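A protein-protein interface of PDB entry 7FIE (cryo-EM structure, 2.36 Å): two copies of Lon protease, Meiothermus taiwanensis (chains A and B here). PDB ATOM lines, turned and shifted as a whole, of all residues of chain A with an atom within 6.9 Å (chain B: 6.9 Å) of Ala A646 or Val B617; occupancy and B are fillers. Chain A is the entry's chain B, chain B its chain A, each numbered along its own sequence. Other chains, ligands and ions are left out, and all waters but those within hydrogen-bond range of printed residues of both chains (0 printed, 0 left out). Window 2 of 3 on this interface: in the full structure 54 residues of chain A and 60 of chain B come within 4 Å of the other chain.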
ATOM      1  N   LEU A 641      -7.386 -17.089  14.550  1.00  0.00           N
ATOM      2  CA  LEU A 641      -6.569 -16.222  13.710  1.00  0.00           C
ATOM      3  C   LEU A 641      -5.434 -15.585  14.501  1.00  0.00           C
ATOM      4  O   LEU A 641      -4.330 -15.419  13.976  1.00  0.00           O
ATOM      5  CB  LEU A 641      -7.441 -15.155  13.062  1.00  0.00           C
ATOM      6  CG  LEU A 641      -6.738 -14.185  12.123  1.00  0.00           C
ATOM      7  CD1 LEU A 641      -6.127 -14.950  10.989  1.00  0.00           C
ATOM      8  CD2 LEU A 641      -7.709 -13.163  11.611  1.00  0.00           C
ATOM      9  N   THR A 642      -5.671 -15.249  15.770  1.00  0.00           N
ATOM     10  CA  THR A 642      -4.605 -14.678  16.586  1.00  0.00           C
ATOM     11  C   THR A 642      -3.553 -15.725  16.930  1.00  0.00           C
ATOM     12  O   THR A 642      -2.361 -15.410  17.005  1.00  0.00           O
ATOM     13  CB  THR A 642      -5.194 -14.060  17.849  1.00  0.00           C
ATOM     14  OG1 THR A 642      -6.194 -13.112  17.474  1.00  0.00           O
ATOM     15  CG2 THR A 642      -4.143 -13.325  18.643  1.00  0.00           C
ATOM     16  N   TYR A 643      -3.970 -16.980  17.115  1.00  0.00           N
ATOM     17  CA  TYR A 643      -2.997 -18.054  17.289  1.00  0.00           C
ATOM     18  C   TYR A 643      -2.132 -18.236  16.052  1.00  0.00           C
ATOM     19  O   TYR A 643      -0.924 -18.455  16.166  1.00  0.00           O
ATOM     20  CB  TYR A 643      -3.683 -19.371  17.628  1.00  0.00           C
ATOM     21  CG  TYR A 643      -2.713 -20.529  17.648  1.00  0.00           C
ATOM     22  CD1 TYR A 643      -1.794 -20.666  18.670  1.00  0.00           C
ATOM     23  CD2 TYR A 643      -2.711 -21.478  16.638  1.00  0.00           C
ATOM     24  CE1 TYR A 643      -0.905 -21.708  18.684  1.00  0.00           C
ATOM     25  CE2 TYR A 643      -1.823 -22.516  16.645  1.00  0.00           C
ATOM     26  CZ  TYR A 643      -0.925 -22.626  17.670  1.00  0.00           C
ATOM     27  OH  TYR A 643      -0.038 -23.669  17.685  1.00  0.00           O
ATOM     28  N   LEU A 644      -2.726 -18.162  14.864  1.00  0.00           N
ATOM     29  CA  LEU A 644      -1.923 -18.358  13.663  1.00  0.00           C
ATOM     30  C   LEU A 644      -1.016 -17.180  13.342  1.00  0.00           C
ATOM     31  O   LEU A 644      -0.036 -17.362  12.619  1.00  0.00           O
ATOM     32  CB  LEU A 644      -2.817 -18.652  12.466  1.00  0.00           C
ATOM     33  CG  LEU A 644      -3.493 -20.015  12.507  1.00  0.00           C
ATOM     34  CD1 LEU A 644      -4.489 -20.134  11.401  1.00  0.00           C
ATOM     35  CD2 LEU A 644      -2.458 -21.098  12.391  1.00  0.00           C
ATOM     36  N   ARG A 645      -1.303 -15.984  13.855  1.00  0.00           N
ATOM     37  CA  ARG A 645      -0.430 -14.845  13.594  1.00  0.00           C
ATOM     38  C   ARG A 645       0.854 -14.894  14.402  1.00  0.00           C
ATOM     39  O   ARG A 645       1.807 -14.194  14.063  1.00  0.00           O
ATOM     40  CB  ARG A 645      -1.152 -13.534  13.887  1.00  0.00           C
ATOM     41  CG  ARG A 645      -2.198 -13.169  12.877  1.00  0.00           C
ATOM     42  CD  ARG A 645      -2.974 -11.942  13.281  1.00  0.00           C
ATOM     43  NE  ARG A 645      -2.156 -10.740  13.303  1.00  0.00           N
ATOM     44  CZ  ARG A 645      -2.585  -9.565  13.741  1.00  0.00           C
ATOM     45  NH1 ARG A 645      -3.823  -9.438  14.182  1.00  0.00           N
ATOM     46  NH2 ARG A 645      -1.780  -8.517  13.733  1.00  0.00           N
ATOM     47  N   ALA A 646       0.900 -15.694  15.458  1.00  0.00           N
ATOM     48  CA  ALA A 646       2.062 -15.754  16.325  1.00  0.00           C
ATOM     49  C   ALA A 646       2.967 -16.938  16.033  1.00  0.00           C
ATOM     50  O   ALA A 646       4.009 -17.070  16.676  1.00  0.00           O
ATOM     51  CB  ALA A 646       1.620 -15.806  17.786  1.00  0.00           C
ATOM     52  N   HIS A 647       2.596 -17.799  15.095  1.00  0.00           N
ATOM     53  CA  HIS A 647       3.383 -18.971  14.744  1.00  0.00           C
ATOM     54  C   HIS A 647       3.483 -19.071  13.232  1.00  0.00           C
ATOM     55  O   HIS A 647       3.271 -20.125  12.636  1.00  0.00           O
ATOM     56  CB  HIS A 647       2.775 -20.237  15.330  1.00  0.00           C
ATOM     57  CG  HIS A 647       2.780 -20.268  16.823  1.00  0.00           C
ATOM     58  ND1 HIS A 647       1.766 -19.728  17.579  1.00  0.00           N
ATOM     59  CD2 HIS A 647       3.675 -20.775  17.700  1.00  0.00           C
ATOM     60  CE1 HIS A 647       2.036 -19.898  18.859  1.00  0.00           C
ATOM     61  NE2 HIS A 647       3.189 -20.530  18.960  1.00  0.00           N
ATOM     62  N   THR A 648       3.819 -17.956  12.592  1.00  0.00           N
ATOM     63  CA  THR A 648       3.722 -17.824  11.145  1.00  0.00           C
ATOM     64  C   THR A 648       4.840 -18.538  10.400  1.00  0.00           C
ATOM     65  O   THR A 648       4.804 -18.603   9.168  1.00  0.00           O
ATOM     66  CB  THR A 648       3.695 -16.348  10.762  1.00  0.00           C
ATOM     67  OG1 THR A 648       3.438 -16.230   9.363  1.00  0.00           O
ATOM     68  CG2 THR A 648       5.024 -15.709  11.072  1.00  0.00           C
ATOM     69  N   GLN A 649       5.823 -19.074  11.096  1.00  0.00           N
ATOM     70  CA  GLN A 649       6.858 -19.834  10.408  1.00  0.00           C
ATOM     71  C   GLN A 649       6.873 -21.297  10.801  1.00  0.00           C
ATOM     72  O   GLN A 649       7.627 -22.064  10.198  1.00  0.00           O
ATOM     73  CB  GLN A 649       8.236 -19.217  10.666  1.00  0.00           C
ATOM     74  CG  GLN A 649       8.757 -19.421  12.069  1.00  0.00           C
ATOM     75  CD  GLN A 649       8.308 -18.341  13.032  1.00  0.00           C
ATOM     76  OE1 GLN A 649       7.364 -17.599  12.763  1.00  0.00           O
ATOM     77  NE2 GLN A 649       8.994 -18.242  14.164  1.00  0.00           N
ATOM     78  N   ASP A 650       6.081 -21.715  11.783  1.00  0.00           N
ATOM     79  CA  ASP A 650       5.931 -23.130  12.069  1.00  0.00           C
ATOM     80  C   ASP A 650       5.135 -23.852  10.999  1.00  0.00           C
ATOM     81  O   ASP A 650       5.301 -25.063  10.836  1.00  0.00           O
ATOM     82  CB  ASP A 650       5.248 -23.321  13.417  1.00  0.00           C
ATOM     83  CG  ASP A 650       6.109 -22.874  14.565  1.00  0.00           C
ATOM     84  OD1 ASP A 650       7.346 -22.917  14.421  1.00  0.00           O
ATOM     85  OD2 ASP A 650       5.556 -22.480  15.610  1.00  0.00           O
ATOM     86  N   PHE A 657       0.624 -11.275   6.611  1.00  0.00           N
ATOM     87  CA  PHE A 657      -0.692 -11.371   6.008  1.00  0.00           C
ATOM     88  C   PHE A 657      -1.666 -10.530   6.807  1.00  0.00           C
ATOM     89  O   PHE A 657      -2.824 -10.379   6.416  1.00  0.00           O
ATOM     90  CB  PHE A 657      -1.154 -12.828   5.914  1.00  0.00           C
ATOM     91  CG  PHE A 657      -1.267 -13.532   7.236  1.00  0.00           C
ATOM     92  CD1 PHE A 657      -0.184 -14.206   7.760  1.00  0.00           C
ATOM     93  CD2 PHE A 657      -2.463 -13.562   7.934  1.00  0.00           C
ATOM     94  CE1 PHE A 657      -0.278 -14.862   8.956  1.00  0.00           C
ATOM     95  CE2 PHE A 657      -2.556 -14.210   9.139  1.00  0.00           C
ATOM     96  CZ  PHE A 657      -1.463 -14.863   9.646  1.00  0.00           C
ATOM     97  N   LEU A 708      -6.162 -19.387  23.120  1.00  0.00           N
ATOM     98  CA  LEU A 708      -5.208 -18.486  22.503  1.00  0.00           C
ATOM     99  C   LEU A 708      -3.793 -19.042  22.527  1.00  0.00           C
ATOM    100  O   LEU A 708      -2.982 -18.677  21.674  1.00  0.00           O
ATOM    101  CB  LEU A 708      -5.275 -17.132  23.203  1.00  0.00           C
ATOM    102  CG  LEU A 708      -4.613 -15.962  22.509  1.00  0.00           C
ATOM    103  CD1 LEU A 708      -5.296 -15.804  21.196  1.00  0.00           C
ATOM    104  CD2 LEU A 708      -4.774 -14.721  23.331  1.00  0.00           C
ATOM    105  N   ALA B 615      -1.822 -12.294  24.005  1.00  0.00           N
ATOM    106  CA  ALA B 615      -0.867 -12.525  22.935  1.00  0.00           C
ATOM    107  C   ALA B 615      -0.456 -11.189  22.349  1.00  0.00           C
ATOM    108  O   ALA B 615      -1.306 -10.332  22.109  1.00  0.00           O
ATOM    109  CB  ALA B 615      -1.462 -13.417  21.849  1.00  0.00           C
ATOM    110  N   ALA B 616       0.836 -11.014  22.125  1.00  0.00           N
ATOM    111  CA  ALA B 616       1.380  -9.806  21.520  1.00  0.00           C
ATOM    112  C   ALA B 616       1.937 -10.171  20.152  1.00  0.00           C
ATOM    113  O   ALA B 616       2.971 -10.833  20.053  1.00  0.00           O
ATOM    114  CB  ALA B 616       2.456  -9.190  22.404  1.00  0.00           C
ATOM    115  N   VAL B 617       1.254  -9.735  19.106  1.00  0.00           N
ATOM    116  CA  VAL B 617       1.646 -10.028  17.731  1.00  0.00           C
ATOM    117  C   VAL B 617       1.968  -8.699  17.068  1.00  0.00           C
ATOM    118  O   VAL B 617       1.486  -7.647  17.515  1.00  0.00           O
ATOM    119  CB  VAL B 617       0.544 -10.812  16.983  1.00  0.00           C
ATOM    120  CG1 VAL B 617       0.369 -12.162  17.610  1.00  0.00           C
ATOM    121  CG2 VAL B 617      -0.750 -10.061  17.036  1.00  0.00           C
ATOM    122  N   PRO B 618       2.811  -8.691  16.030  1.00  0.00           N
ATOM    123  CA  PRO B 618       3.111  -7.423  15.354  1.00  0.00           C
ATOM    124  C   PRO B 618       1.908  -6.898  14.590  1.00  0.00           C
ATOM    125  O   PRO B 618       1.284  -7.618  13.813  1.00  0.00           O
ATOM    126  CB  PRO B 618       4.264  -7.784  14.415  1.00  0.00           C
ATOM    127  CG  PRO B 618       4.158  -9.224  14.228  1.00  0.00           C
ATOM    128  CD  PRO B 618       3.671  -9.771  15.521  1.00  0.00           C
ATOM    129  N   GLY B 619       1.579  -5.637  14.840  1.00  0.00           N
ATOM    130  CA  GLY B 619       0.423  -5.008  14.239  1.00  0.00           C
ATOM    131  C   GLY B 619       0.556  -3.504  14.178  1.00  0.00           C
ATOM    132  O   GLY B 619       1.629  -2.990  13.860  1.00  0.00           O
ATOM    133  N   SER B 620      -0.520  -2.784  14.486  1.00  0.00           N
ATOM    134  CA  SER B 620      -0.506  -1.332  14.373  1.00  0.00           C
ATOM    135  C   SER B 620      -0.997  -0.678  15.653  1.00  0.00           C
ATOM    136  O   SER B 620      -1.057   0.548  15.751  1.00  0.00           O
ATOM    137  CB  SER B 620      -1.367  -0.883  13.199  1.00  0.00           C
ATOM    138  OG  SER B 620      -2.729  -1.166  13.448  1.00  0.00           O
ATOM    139  N   GLY B 621      -1.381  -1.489  16.625  1.00  0.00           N
ATOM    140  CA  GLY B 621      -1.750  -1.004  17.935  1.00  0.00           C
ATOM    141  C   GLY B 621      -3.247  -0.931  18.104  1.00  0.00           C
ATOM    142  O   GLY B 621      -3.870   0.071  17.757  1.00  0.00           O
ATOM    143  N   LYS B 660       2.893  -0.406  17.343  1.00  0.00           N
ATOM    144  CA  LYS B 660       3.567  -1.496  16.652  1.00  0.00           C
ATOM    145  C   LYS B 660       3.043  -2.874  17.005  1.00  0.00           C
ATOM    146  O   LYS B 660       3.357  -3.821  16.282  1.00  0.00           O
ATOM    147  CB  LYS B 660       5.069  -1.470  16.945  1.00  0.00           C
ATOM    148  CG  LYS B 660       5.775  -0.237  16.457  1.00  0.00           C
ATOM    149  CD  LYS B 660       5.760  -0.178  14.950  1.00  0.00           C
ATOM    150  CE  LYS B 660       6.525   1.027  14.444  1.00  0.00           C
ATOM    151  NZ  LYS B 660       6.466   1.122  12.961  1.00  0.00           N
ATOM    152  N   VAL B 661       2.278  -3.031  18.080  1.00  0.00           N
ATOM    153  CA  VAL B 661       1.896  -4.336  18.601  1.00  0.00           C
ATOM    154  C   VAL B 661       0.389  -4.370  18.774  1.00  0.00           C
ATOM    155  O   VAL B 661      -0.179  -3.496  19.433  1.00  0.00           O
ATOM    156  CB  VAL B 661       2.589  -4.630  19.944  1.00  0.00           C
ATOM    157  CG1 VAL B 661       2.067  -5.903  20.540  1.00  0.00           C
ATOM    158  CG2 VAL B 661       4.083  -4.729  19.771  1.00  0.00           C
ATOM    159  N   ASP B 662      -0.258  -5.373  18.189  1.00  0.00           N
ATOM    160  CA  ASP B 662      -1.644  -5.673  18.502  1.00  0.00           C
ATOM    161  C   ASP B 662      -1.701  -6.600  19.704  1.00  0.00           C
ATOM    162  O   ASP B 662      -0.901  -7.528  19.819  1.00  0.00           O
ATOM    163  CB  ASP B 662      -2.351  -6.330  17.320  1.00  0.00           C
ATOM    164  CG  ASP B 662      -2.532  -5.394  16.152  1.00  0.00           C
ATOM    165  OD1 ASP B 662      -2.552  -4.168  16.367  1.00  0.00           O
ATOM    166  OD2 ASP B 662      -2.680  -5.881  15.015  1.00  0.00           O
ATOM    167  N   LEU B 663      -2.646  -6.345  20.600  1.00  0.00           N
ATOM    168  CA  LEU B 663      -2.840  -7.165  21.786  1.00  0.00           C
ATOM    169  C   LEU B 663      -4.222  -7.785  21.753  1.00  0.00           C
ATOM    170  O   LEU B 663      -5.206  -7.102  21.469  1.00  0.00           O
ATOM    171  CB  LEU B 663      -2.685  -6.356  23.066  1.00  0.00           C
ATOM    172  CG  LEU B 663      -1.302  -5.849  23.433  1.00  0.00           C
ATOM    173  CD1 LEU B 663      -1.417  -4.981  24.647  1.00  0.00           C
ATOM    174  CD2 LEU B 663      -0.393  -7.006  23.713  1.00  0.00           C
ATOM    175  N   HIS B 664      -4.294  -9.070  22.066  1.00  0.00           N
ATOM    176  CA  HIS B 664      -5.547  -9.803  22.122  1.00  0.00           C
ATOM    177  C   HIS B 664      -5.657 -10.451  23.488  1.00  0.00           C
ATOM    178  O   HIS B 664      -4.792 -11.239  23.869  1.00  0.00           O
ATOM    179  CB  HIS B 664      -5.602 -10.861  21.026  1.00  0.00           C
ATOM    180  CG  HIS B 664      -6.876 -11.637  20.993  1.00  0.00           C
ATOM    181  ND1 HIS B 664      -8.029 -11.157  20.420  1.00  0.00           N
ATOM    182  CD2 HIS B 664      -7.186 -12.857  21.482  1.00  0.00           C
ATOM    183  CE1 HIS B 664      -8.989 -12.052  20.544  1.00  0.00           C
ATOM    184  NE2 HIS B 664      -8.504 -13.093  21.189  1.00  0.00           N
ATOM    185  N   ARG B 693       8.158 -10.638  27.493  1.00  0.00           N
ATOM    186  CA  ARG B 693       8.606 -12.002  27.190  1.00  0.00           C
ATOM    187  C   ARG B 693       9.161 -12.736  28.407  1.00  0.00           C
ATOM    188  O   ARG B 693       9.971 -13.650  28.267  1.00  0.00           O
ATOM    189  CB  ARG B 693       9.630 -12.024  26.054  1.00  0.00           C
ATOM    190  CG  ARG B 693       9.087 -11.528  24.752  1.00  0.00           C
ATOM    191  CD  ARG B 693       8.033 -12.481  24.277  1.00  0.00           C
ATOM    192  NE  ARG B 693       7.515 -12.138  22.963  1.00  0.00           N
ATOM    193  CZ  ARG B 693       6.524 -12.791  22.372  1.00  0.00           C
ATOM    194  NH1 ARG B 693       5.948 -13.812  22.987  1.00  0.00           N
ATOM    195  NH2 ARG B 693       6.106 -12.424  21.171  1.00  0.00           N
ATOM    196  N   VAL B 779       8.807  -9.054  20.447  1.00  0.00           N
ATOM    197  CA  VAL B 779       7.658  -9.019  19.547  1.00  0.00           C
ATOM    198  C   VAL B 779       8.019  -8.317  18.248  1.00  0.00           C
ATOM    199  O   VAL B 779       7.775  -8.838  17.153  1.00  0.00           O
ATOM    200  CB  VAL B 779       6.465  -8.337  20.239  1.00  0.00           C
ATOM    201  CG1 VAL B 779       5.267  -8.307  19.310  1.00  0.00           C
ATOM    202  CG2 VAL B 779       6.138  -9.031  21.549  1.00  0.00           C
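O of Pro B618 sits at hydrogen-bond distance from NH2 of Arg A645. The guanidinium group (NH2) of Arg A645 is in salt-bridge range of the side-chain carboxylate (OD2) of Asp B662.
OD1 of Asp B662 sits at hydrogen-bond distance from N of Ser B620 (3.1 Å). The side-chain carboxylate of Asp B662 is in hydrogen-bond range of the backbone NH of Gly B621 (2.9 Å). N of Asp B662 lies within hydrogen-bond range of O of Val B617 (2.9 Å). The backbone NH (N) of Ala B615 lies within hydrogen-bond range of the backbone carbonyl oxygen (O) of His B664 (3.2 Å).
Among the printed residues, pairs that only touch across the chains: Thr A642 with His B664, Arg A645 with Val B617, Ala A646 with Val B617, Leu A708 with Ala B615 and Leu A708 with His B664.
Of chain B, only Val B617 (3.9 Å) comes within 4 Å of Ala A646. Of chain A, only Arg A645 (3.8 Å) and Ala A646 (3.9 Å) come within 4 Å of Val B617. Printed residues of chain B within 4 Å of Thr A642: His B664. Of the printed residues of chain B, Arg A645 touches Val B617, Pro B618 and Asp B662. Printed residues of chain A within 4 Å of His B664: Thr A642 and Leu A708. Thr A648 touches none of the printed residues of chain B. The nearest residue of chain A that does not touch Val B617 is Thr A642 (4.3 Å). The nearest printed residue of chain A that does not touch Asp B662 is Thr A642 (6.7 Å).
Hydrophobic or aromatic side chains of chain A within 4 Å of the printed part of chain B: Ala A646 and Leu A708. Among the printed residues, Asp or Glu carboxylates within 4 Å of a Lys or Arg side-chain nitrogen of the other chain: Arg A645 with Asp B662.
No position is printed for both chains.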
